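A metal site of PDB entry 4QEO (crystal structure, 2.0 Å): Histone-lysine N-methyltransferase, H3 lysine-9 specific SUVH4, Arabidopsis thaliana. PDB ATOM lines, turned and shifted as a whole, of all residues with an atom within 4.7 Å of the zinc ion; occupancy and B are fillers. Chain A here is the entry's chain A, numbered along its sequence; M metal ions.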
ATOM      1  N   HIS A 461     -13.612 -14.776  -5.820  1.00  0.00           N
ATOM      2  CA  HIS A 461     -14.562 -14.711  -4.724  1.00  0.00           C
ATOM      3  C   HIS A 461     -14.156 -15.662  -3.600  1.00  0.00           C
ATOM      4  O   HIS A 461     -13.594 -16.726  -3.840  1.00  0.00           O
ATOM      5  CB  HIS A 461     -15.961 -15.101  -5.222  1.00  0.00           C
ATOM      6  CG  HIS A 461     -16.917 -15.507  -4.128  1.00  0.00           C
ATOM      7  ND1 HIS A 461     -17.823 -14.636  -3.567  1.00  0.00           N
ATOM      8  CD2 HIS A 461     -17.099 -16.694  -3.498  1.00  0.00           C
ATOM      9  CE1 HIS A 461     -18.528 -15.268  -2.634  1.00  0.00           C
ATOM     10  NE2 HIS A 461     -18.104 -16.519  -2.574  1.00  0.00           N
ATOM     11  N   CYS A 463     -15.960 -16.930   0.436  1.00  0.00           N
ATOM     12  CA  CYS A 463     -16.991 -16.794   1.454  1.00  0.00           C
ATOM     13  C   CYS A 463     -16.398 -16.237   2.743  1.00  0.00           C
ATOM     14  O   CYS A 463     -17.123 -15.687   3.572  1.00  0.00           O
ATOM     15  CB  CYS A 463     -17.680 -18.142   1.699  1.00  0.00           C
ATOM     16  SG  CYS A 463     -18.526 -18.842   0.221  1.00  0.00           S
ATOM     17  N   CYS A 521     -19.119 -23.151  -5.751  1.00  0.00           N
ATOM     18  CA  CYS A 521     -18.059 -22.366  -5.145  1.00  0.00           C
ATOM     19  C   CYS A 521     -16.981 -23.236  -4.568  1.00  0.00           C
ATOM     20  O   CYS A 521     -17.197 -24.284  -3.945  1.00  0.00           O
ATOM     21  CB  CYS A 521     -18.582 -21.472  -4.031  1.00  0.00           C
ATOM     22  SG  CYS A 521     -17.293 -20.422  -3.313  1.00  0.00           S
ATOM     23  N   TYR A 522     -15.778 -22.728  -4.753  1.00  0.00           N
ATOM     24  CA  TYR A 522     -14.629 -23.502  -4.411  1.00  0.00           C
ATOM     25  C   TYR A 522     -13.610 -22.642  -3.619  1.00  0.00           C
ATOM     26  O   TYR A 522     -12.381 -22.842  -3.670  1.00  0.00           O
ATOM     27  CB  TYR A 522     -14.071 -24.173  -5.687  1.00  0.00           C
ATOM     28  CG  TYR A 522     -12.573 -24.149  -5.654  1.00  0.00           C
ATOM     29  CD1 TYR A 522     -11.839 -25.071  -4.933  1.00  0.00           C
ATOM     30  CD2 TYR A 522     -11.883 -23.108  -6.271  1.00  0.00           C
ATOM     31  CE1 TYR A 522     -10.495 -24.968  -4.860  1.00  0.00           C
ATOM     32  CE2 TYR A 522     -10.515 -22.992  -6.212  1.00  0.00           C
ATOM     33  CZ  TYR A 522      -9.816 -23.919  -5.545  1.00  0.00           C
ATOM     34  OH  TYR A 522      -8.479 -23.628  -5.584  1.00  0.00           O
ATOM     35  N   CYS A 523     -14.097 -21.704  -2.824  1.00  0.00           N
ATOM     36  CA  CYS A 523     -13.140 -20.873  -2.090  1.00  0.00           C
ATOM     37  C   CYS A 523     -12.382 -21.700  -1.050  1.00  0.00           C
ATOM     38  O   CYS A 523     -11.305 -21.324  -0.595  1.00  0.00           O
ATOM     39  CB  CYS A 523     -13.793 -19.638  -1.480  1.00  0.00           C
ATOM     40  SG  CYS A 523     -14.950 -20.064  -0.203  1.00  0.00           S
ATOM     41  N   CYS A 528     -18.534 -22.500   3.557  1.00  0.00           N
ATOM     42  CA  CYS A 528     -18.546 -22.114   2.157  1.00  0.00           C
ATOM     43  C   CYS A 528     -19.925 -21.839   1.527  1.00  0.00           C
ATOM     44  O   CYS A 528     -20.004 -21.257   0.455  1.00  0.00           O
ATOM     45  CB  CYS A 528     -17.807 -23.191   1.345  1.00  0.00           C
ATOM     46  SG  CYS A 528     -17.709 -22.956  -0.444  1.00  0.00           S
HETATM   47 ZN    ZN M   1     -17.228 -20.652  -0.925  1.00  0.00          ZN
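The side-chain sulfur (SG) of Cys 463 lies close to a ring nitrogen (NE2) of His 461 (3.7 Å).
Within 4 Å of the zinc ion: Cys 463, Cys 521, Cys 523 and Cys 528.
Along chain A the residues within 4 Å of the zinc ion span positions 463 to 528.
The zinc ion is bound by SG of Cys 521 (2.4 Å), SG of Cys 528 (2.4 Å), SG of Cys 523 (2.5 Å) and SG of Cys 463 (2.5 Å).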
